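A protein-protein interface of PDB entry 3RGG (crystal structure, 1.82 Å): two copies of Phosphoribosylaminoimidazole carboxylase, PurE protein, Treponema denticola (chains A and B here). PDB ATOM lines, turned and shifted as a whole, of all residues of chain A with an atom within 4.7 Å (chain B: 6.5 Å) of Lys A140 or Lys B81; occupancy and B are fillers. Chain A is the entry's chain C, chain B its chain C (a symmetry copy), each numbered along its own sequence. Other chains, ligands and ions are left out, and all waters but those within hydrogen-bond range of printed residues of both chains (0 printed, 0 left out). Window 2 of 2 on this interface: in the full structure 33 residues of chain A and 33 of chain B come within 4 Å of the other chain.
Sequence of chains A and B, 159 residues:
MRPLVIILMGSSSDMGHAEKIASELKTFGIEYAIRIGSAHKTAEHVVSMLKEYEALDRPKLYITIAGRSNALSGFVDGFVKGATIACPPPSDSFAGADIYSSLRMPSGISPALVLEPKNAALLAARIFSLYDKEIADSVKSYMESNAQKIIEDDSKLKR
NE of Arg A126 lies within hydrogen-bond range of O of Lys B81 (2.8 Å). NH2 of Arg A126 lies within hydrogen-bond range of O of Val B80 (3.2 Å). NH2 of Arg A126 lies within hydrogen-bond range of O of Gly B82, at 3.0 Å. The side-chain carboxylate (OD2) of Asp B77 is in salt-bridge range of the guanidinium group (NH1) of Arg A126, 2.8 Å away.
NZ of Lys B81 is in salt-bridge range of OE1 of Glu B54 (3.8 Å). The backbone carbonyl oxygen (O) of Arg A126 sits at hydrogen-bond distance from the side-chain hydroxyl (OG) of Ser A129 (2.9 Å).
Ala B83 touches Arg A126 (N to CB, 3.6 Å). Val A139 touches Lys B81. Lys B81 touches Lys A140 (NZ to NZ, 3.6 Å). Asp B77 touches Met A143.
Of the printed residues of chain B, Val A139 touches Lys B81 (3.7 Å). Lys A140 touches just one residue of chain B: Lys B81 (3.6 Å). Ser A141 touches none of the printed residues of chain B. Of the printed residues of chain A, Val B80 touches Arg A126. Lys B81 touches just these residues of chain A: Arg A126 (2.8 Å), Val A139 (3.7 Å) and Lys A140 (3.6 Å). Printed residues of chain A within 4 Å of Ala B83: Arg A126 (3.6 Å). The nearest printed residue of chain B that does not touch Lys A140 is Glu B54 (6.7 Å). The nearest residue of chain A that does not touch Lys B81 is Met A143 (4.4 Å). The nearest printed residue of chain A that does not touch Val B80 is Met A143 (4.3 Å).
Printed residues of chain A that touch a printed residue of chain B: Arg A126, Val A139, Lys A140 and Met A143. Along chain A the printed residues that touch a printed residue of chain B span positions 126 to 143. Printed residues of chain B that touch a printed residue of chain A: Asp B77, Val B80, Lys B81, Gly B82 and Ala B83. Hydrophobic or aromatic side chains of chain B within 4 Å of the printed part of chain A: Ala B83. Along chain B the printed residues that touch a printed residue of chain A span positions 77 to 83. Among the printed residues, 8 pairs touch across the chains. Among the printed residues, Asp or Glu carboxylates within 4 Å of a Lys or Arg side-chain nitrogen of the other chain: Arg A126 with Asp B77 (2.8 Å).
No position is printed for both chains. Of the 8 pairs that touch across the chains among the printed residues, none has its exchanged pair printed and touching as well.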
ATOM      1  N   ARG A 126      30.693   1.575 -32.829  1.00  0.00           N
ATOM      2  CA  ARG A 126      30.760   1.241 -31.407  1.00  0.00           C
ATOM      3  C   ARG A 126      31.593   2.245 -30.588  1.00  0.00           C
ATOM      4  O   ARG A 126      31.402   2.352 -29.373  1.00  0.00           O
ATOM      5  CB  ARG A 126      31.237  -0.190 -31.204  1.00  0.00           C
ATOM      6  CG  ARG A 126      30.306  -1.198 -31.857  1.00  0.00           C
ATOM      7  CD  ARG A 126      30.992  -2.537 -32.100  1.00  0.00           C
ATOM      8  NE  ARG A 126      31.124  -3.287 -30.855  1.00  0.00           N
ATOM      9  CZ  ARG A 126      31.603  -4.514 -30.767  1.00  0.00           C
ATOM     10  NH1 ARG A 126      32.027  -5.134 -31.853  1.00  0.00           N
ATOM     11  NH2 ARG A 126      31.686  -5.113 -29.584  1.00  0.00           N
ATOM     12  N   SER A 129      29.026   4.803 -29.882  1.00  0.00           N
ATOM     13  CA  SER A 129      27.964   4.234 -29.034  1.00  0.00           C
ATOM     14  C   SER A 129      28.201   4.315 -27.546  1.00  0.00           C
ATOM     15  O   SER A 129      27.290   4.061 -26.769  1.00  0.00           O
ATOM     16  CB  SER A 129      27.747   2.754 -29.368  1.00  0.00           C
ATOM     17  OG  SER A 129      28.661   1.919 -28.673  1.00  0.00           O
ATOM     18  N   ALA A 136      24.220   3.308 -30.481  1.00  0.00           N
ATOM     19  CA  ALA A 136      24.224   2.166 -29.568  1.00  0.00           C
ATOM     20  C   ALA A 136      23.061   1.214 -29.841  1.00  0.00           C
ATOM     21  O   ALA A 136      23.270   0.010 -29.939  1.00  0.00           O
ATOM     22  CB  ALA A 136      24.166   2.668 -28.108  1.00  0.00           C
ATOM     23  N   ASP A 137      21.839   1.755 -29.965  1.00  0.00           N
ATOM     24  CA  ASP A 137      20.656   0.931 -30.291  1.00  0.00           C
ATOM     25  C   ASP A 137      20.797   0.226 -31.649  1.00  0.00           C
ATOM     26  O   ASP A 137      20.417  -0.931 -31.808  1.00  0.00           O
ATOM     27  CB  ASP A 137      19.360   1.767 -30.236  1.00  0.00           C
ATOM     28  CG  ASP A 137      19.016   2.230 -28.806  1.00  0.00           C
ATOM     29  OD1 ASP A 137      19.822   1.985 -27.870  1.00  0.00           O
ATOM     30  OD2 ASP A 137      17.938   2.849 -28.615  1.00  0.00           O
ATOM     31  N   SER A 138      21.384   0.903 -32.624  1.00  0.00           N
ATOM     32  CA  SER A 138      21.537   0.311 -33.949  1.00  0.00           C
ATOM     33  C   SER A 138      22.637  -0.775 -34.029  1.00  0.00           C
ATOM     34  O   SER A 138      22.430  -1.768 -34.722  1.00  0.00           O
ATOM     35  CB  SER A 138      21.745   1.401 -35.001  1.00  0.00           C
ATOM     36  OG  SER A 138      22.220   0.835 -36.204  1.00  0.00           O
ATOM     37  N   VAL A 139      23.759  -0.589 -33.313  1.00  0.00           N
ATOM     38  CA  VAL A 139      24.784  -1.636 -33.149  1.00  0.00           C
ATOM     39  C   VAL A 139      24.164  -2.824 -32.423  1.00  0.00           C
ATOM     40  O   VAL A 139      24.354  -3.953 -32.844  1.00  0.00           O
ATOM     41  CB  VAL A 139      26.052  -1.116 -32.361  1.00  0.00           C
ATOM     42  CG1 VAL A 139      26.939  -2.277 -31.874  1.00  0.00           C
ATOM     43  CG2 VAL A 139      26.829  -0.098 -33.187  1.00  0.00           C
ATOM     44  N   LYS A 140      23.406  -2.583 -31.348  1.00  0.00           N
ATOM     45  CA  LYS A 140      22.766  -3.688 -30.626  1.00  0.00           C
ATOM     46  C   LYS A 140      21.934  -4.550 -31.592  1.00  0.00           C
ATOM     47  O   LYS A 140      22.057  -5.776 -31.573  1.00  0.00           O
ATOM     48  CB  LYS A 140      21.908  -3.181 -29.429  1.00  0.00           C
ATOM     49  CG  LYS A 140      21.136  -4.251 -28.598  1.00  0.00           C
ATOM     50  CD  LYS A 140      20.311  -3.617 -27.411  1.00  0.00           C
ATOM     51  CE  LYS A 140      21.131  -3.546 -26.084  1.00  0.00           C
ATOM     52  NZ  LYS A 140      22.662  -3.422 -26.292  1.00  0.00           N
ATOM     53  N   SER A 141      21.120  -3.918 -32.439  1.00  0.00           N
ATOM     54  CA  SER A 141      20.232  -4.642 -33.374  1.00  0.00           C
ATOM     55  C   SER A 141      20.997  -5.441 -34.406  1.00  0.00           C
ATOM     56  O   SER A 141      20.674  -6.587 -34.703  1.00  0.00           O
ATOM     57  CB  SER A 141      19.278  -3.673 -34.117  1.00  0.00           C
ATOM     58  OG  SER A 141      18.083  -3.497 -33.401  1.00  0.00           O
ATOM     59  N   TYR A 142      22.025  -4.816 -34.954  1.00  0.00           N
ATOM     60  CA  TYR A 142      22.903  -5.440 -35.929  1.00  0.00           C
ATOM     61  C   TYR A 142      23.593  -6.701 -35.406  1.00  0.00           C
ATOM     62  O   TYR A 142      23.591  -7.743 -36.068  1.00  0.00           O
ATOM     63  CB  TYR A 142      23.939  -4.396 -36.309  1.00  0.00           C
ATOM     64  CG  TYR A 142      24.958  -4.758 -37.370  1.00  0.00           C
ATOM     65  CD1 TYR A 142      24.623  -4.719 -38.720  1.00  0.00           C
ATOM     66  CD2 TYR A 142      26.273  -5.024 -37.025  1.00  0.00           C
ATOM     67  CE1 TYR A 142      25.548  -5.001 -39.684  1.00  0.00           C
ATOM     68  CE2 TYR A 142      27.223  -5.331 -37.988  1.00  0.00           C
ATOM     69  CZ  TYR A 142      26.855  -5.308 -39.319  1.00  0.00           C
ATOM     70  OH  TYR A 142      27.810  -5.571 -40.278  1.00  0.00           O
ATOM     71  N   MET A 143      24.216  -6.588 -34.230  1.00  0.00           N
ATOM     72  CA  MET A 143      25.029  -7.677 -33.675  1.00  0.00           C
ATOM     73  C   MET A 143      24.118  -8.821 -33.248  1.00  0.00           C
ATOM     74  O   MET A 143      24.449  -9.987 -33.467  1.00  0.00           O
ATOM     75  CB  MET A 143      25.886  -7.191 -32.500  1.00  0.00           C
ATOM     76  CG  MET A 143      26.963  -6.176 -32.917  1.00  0.00           C
ATOM     77  SD  MET A 143      28.272  -5.834 -31.715  1.00  0.00           S
ATOM     78  CE  MET A 143      29.073  -7.448 -31.716  1.00  0.00           C
ATOM     79  N   GLU A 144      22.969  -8.494 -32.652  1.00  0.00           N
ATOM     80  CA  GLU A 144      21.993  -9.527 -32.291  1.00  0.00           C
ATOM     81  C   GLU A 144      21.501 -10.274 -33.516  1.00  0.00           C
ATOM     82  O   GLU A 144      21.323 -11.484 -33.458  1.00  0.00           O
ATOM     83  CB  GLU A 144      20.813  -8.978 -31.465  1.00  0.00           C
ATOM     84  CG  GLU A 144      21.203  -8.749 -29.992  1.00  0.00           C
ATOM     85  CD  GLU A 144      20.074  -8.188 -29.116  1.00  0.00           C
ATOM     86  OE1 GLU A 144      18.881  -8.127 -29.534  1.00  0.00           O
ATOM     87  OE2 GLU A 144      20.404  -7.805 -27.978  1.00  0.00           O
ATOM     88  N   GLU B  54      29.169  -4.973 -18.226  1.00  0.00           N
ATOM     89  CA  GLU B  54      28.214  -4.467 -19.185  1.00  0.00           C
ATOM     90  C   GLU B  54      27.055  -3.805 -18.473  1.00  0.00           C
ATOM     91  O   GLU B  54      26.547  -2.811 -18.961  1.00  0.00           O
ATOM     92  CB  GLU B  54      27.725  -5.579 -20.102  1.00  0.00           C
ATOM     93  CG  GLU B  54      28.783  -5.988 -21.082  1.00  0.00           C
ATOM     94  CD  GLU B  54      29.099  -4.892 -22.072  1.00  0.00           C
ATOM     95  OE1 GLU B  54      28.363  -4.815 -23.059  1.00  0.00           O
ATOM     96  OE2 GLU B  54      30.077  -4.116 -21.884  1.00  0.00           O
ATOM     97  N   ALA B  55      26.679  -4.342 -17.308  1.00  0.00           N
ATOM     98  CA  ALA B  55      25.606  -3.792 -16.494  1.00  0.00           C
ATOM     99  C   ALA B  55      25.836  -2.375 -15.956  1.00  0.00           C
ATOM    100  O   ALA B  55      24.887  -1.728 -15.519  1.00  0.00           O
ATOM    101  CB  ALA B  55      25.305  -4.740 -15.320  1.00  0.00           C
ATOM    102  N   LYS B  60      32.479   2.722 -21.442  1.00  0.00           N
ATOM    103  CA  LYS B  60      33.561   1.756 -21.212  1.00  0.00           C
ATOM    104  C   LYS B  60      34.182   1.156 -22.435  1.00  0.00           C
ATOM    105  O   LYS B  60      33.543   1.020 -23.496  1.00  0.00           O
ATOM    106  CB  LYS B  60      33.068   0.616 -20.321  1.00  0.00           C
ATOM    107  CG  LYS B  60      32.012  -0.295 -20.975  1.00  0.00           C
ATOM    108  CD  LYS B  60      31.215  -1.096 -19.930  1.00  0.00           C
ATOM    109  CE  LYS B  60      30.115  -0.306 -19.266  1.00  0.00           C
ATOM    110  NZ  LYS B  60      28.979   0.051 -20.169  1.00  0.00           N
ATOM    111  N   TYR B  62      37.078  -2.222 -23.355  1.00  0.00           N
ATOM    112  CA  TYR B  62      37.858  -3.347 -22.903  1.00  0.00           C
ATOM    113  C   TYR B  62      39.131  -3.387 -23.743  1.00  0.00           C
ATOM    114  O   TYR B  62      39.086  -3.197 -24.959  1.00  0.00           O
ATOM    115  CB  TYR B  62      37.078  -4.662 -23.031  1.00  0.00           C
ATOM    116  CG  TYR B  62      35.752  -4.683 -22.314  1.00  0.00           C
ATOM    117  CD1 TYR B  62      34.666  -4.004 -22.833  1.00  0.00           C
ATOM    118  CD2 TYR B  62      35.572  -5.406 -21.133  1.00  0.00           C
ATOM    119  CE1 TYR B  62      33.421  -4.009 -22.182  1.00  0.00           C
ATOM    120  CE2 TYR B  62      34.344  -5.425 -20.481  1.00  0.00           C
ATOM    121  CZ  TYR B  62      33.284  -4.717 -20.993  1.00  0.00           C
ATOM    122  OH  TYR B  62      32.081  -4.752 -20.349  1.00  0.00           O
ATOM    123  N   VAL B  76      35.479 -11.596 -26.376  1.00  0.00           N
ATOM    124  CA  VAL B  76      35.015 -10.440 -25.617  1.00  0.00           C
ATOM    125  C   VAL B  76      34.269  -9.514 -26.550  1.00  0.00           C
ATOM    126  O   VAL B  76      33.177  -9.036 -26.229  1.00  0.00           O
ATOM    127  CB  VAL B  76      36.197  -9.708 -24.967  1.00  0.00           C
ATOM    128  CG1 VAL B  76      35.770  -8.414 -24.394  1.00  0.00           C
ATOM    129  CG2 VAL B  76      36.828 -10.596 -23.889  1.00  0.00           C
ATOM    130  N   ASP B  77      34.857  -9.279 -27.729  1.00  0.00           N
ATOM    131  CA  ASP B  77      34.311  -8.287 -28.653  1.00  0.00           C
ATOM    132  C   ASP B  77      32.903  -8.649 -29.103  1.00  0.00           C
ATOM    133  O   ASP B  77      32.032  -7.777 -29.263  1.00  0.00           O
ATOM    134  CB  ASP B  77      35.169  -8.103 -29.884  1.00  0.00           C
ATOM    135  CG  ASP B  77      34.672  -6.977 -30.741  1.00  0.00           C
ATOM    136  OD1 ASP B  77      35.048  -5.830 -30.461  1.00  0.00           O
ATOM    137  OD2 ASP B  77      33.879  -7.221 -31.679  1.00  0.00           O
ATOM    138  N   GLY B  78      32.688  -9.943 -29.298  1.00  0.00           N
ATOM    139  CA  GLY B  78      31.394 -10.455 -29.731  1.00  0.00           C
ATOM    140  C   GLY B  78      30.342 -10.452 -28.637  1.00  0.00           C
ATOM    141  O   GLY B  78      29.135 -10.351 -28.928  1.00  0.00           O
ATOM    142  N   PHE B  79      30.789 -10.546 -27.381  1.00  0.00           N
ATOM    143  CA  PHE B  79      29.870 -10.537 -26.264  1.00  0.00           C
ATOM    144  C   PHE B  79      29.376  -9.117 -25.887  1.00  0.00           C
ATOM    145  O   PHE B  79      28.189  -8.901 -25.663  1.00  0.00           O
ATOM    146  CB  PHE B  79      30.518 -11.212 -25.034  1.00  0.00           C
ATOM    147  CG  PHE B  79      29.532 -11.447 -23.928  1.00  0.00           C
ATOM    148  CD1 PHE B  79      28.775 -12.619 -23.884  1.00  0.00           C
ATOM    149  CD2 PHE B  79      29.280 -10.461 -22.997  1.00  0.00           C
ATOM    150  CE1 PHE B  79      27.847 -12.817 -22.905  1.00  0.00           C
ATOM    151  CE2 PHE B  79      28.344 -10.652 -22.013  1.00  0.00           C
ATOM    152  CZ  PHE B  79      27.613 -11.832 -21.976  1.00  0.00           C
ATOM    153  N   VAL B  80      30.298  -8.167 -25.780  1.00  0.00           N
ATOM    154  CA  VAL B  80      29.987  -6.814 -25.297  1.00  0.00           C
ATOM    155  C   VAL B  80      29.432  -5.975 -26.464  1.00  0.00           C
ATOM    156  O   VAL B  80      29.506  -6.382 -27.608  1.00  0.00           O
ATOM    157  CB  VAL B  80      31.231  -6.175 -24.613  1.00  0.00           C
ATOM    158  CG1 VAL B  80      31.879  -7.183 -23.591  1.00  0.00           C
ATOM    159  CG2 VAL B  80      32.269  -5.713 -25.643  1.00  0.00           C
ATOM    160  N   LYS B  81      28.847  -4.815 -26.190  1.00  0.00           N
ATOM    161  CA  LYS B  81      28.231  -4.037 -27.286  1.00  0.00           C
ATOM    162  C   LYS B  81      29.081  -2.834 -27.716  1.00  0.00           C
ATOM    163  O   LYS B  81      29.197  -2.575 -28.934  1.00  0.00           O
ATOM    164  CB  LYS B  81      26.774  -3.658 -27.013  1.00  0.00           C
ATOM    165  CG  LYS B  81      26.276  -3.801 -25.608  1.00  0.00           C
ATOM    166  CD  LYS B  81      26.664  -2.612 -24.692  1.00  0.00           C
ATOM    167  CE  LYS B  81      26.015  -2.732 -23.315  1.00  0.00           C
ATOM    168  NZ  LYS B  81      24.805  -3.585 -23.395  1.00  0.00           N
ATOM    169  N   GLY B  82      29.753  -2.188 -26.751  1.00  0.00           N
ATOM    170  CA  GLY B  82      30.707  -1.118 -27.018  1.00  0.00           C
ATOM    171  C   GLY B  82      32.027  -1.622 -27.622  1.00  0.00           C
ATOM    172  O   GLY B  82      32.272  -2.824 -27.663  1.00  0.00           O
ATOM    173  N   ALA B  83      32.880  -0.697 -28.069  1.00  0.00           N
ATOM    174  CA  ALA B  83      34.147  -1.026 -28.744  1.00  0.00           C
ATOM    175  C   ALA B  83      35.105  -1.735 -27.819  1.00  0.00           C
ATOM    176  O   ALA B  83      35.006  -1.623 -26.573  1.00  0.00           O
ATOM    177  CB  ALA B  83      34.812   0.241 -29.349  1.00  0.00           C
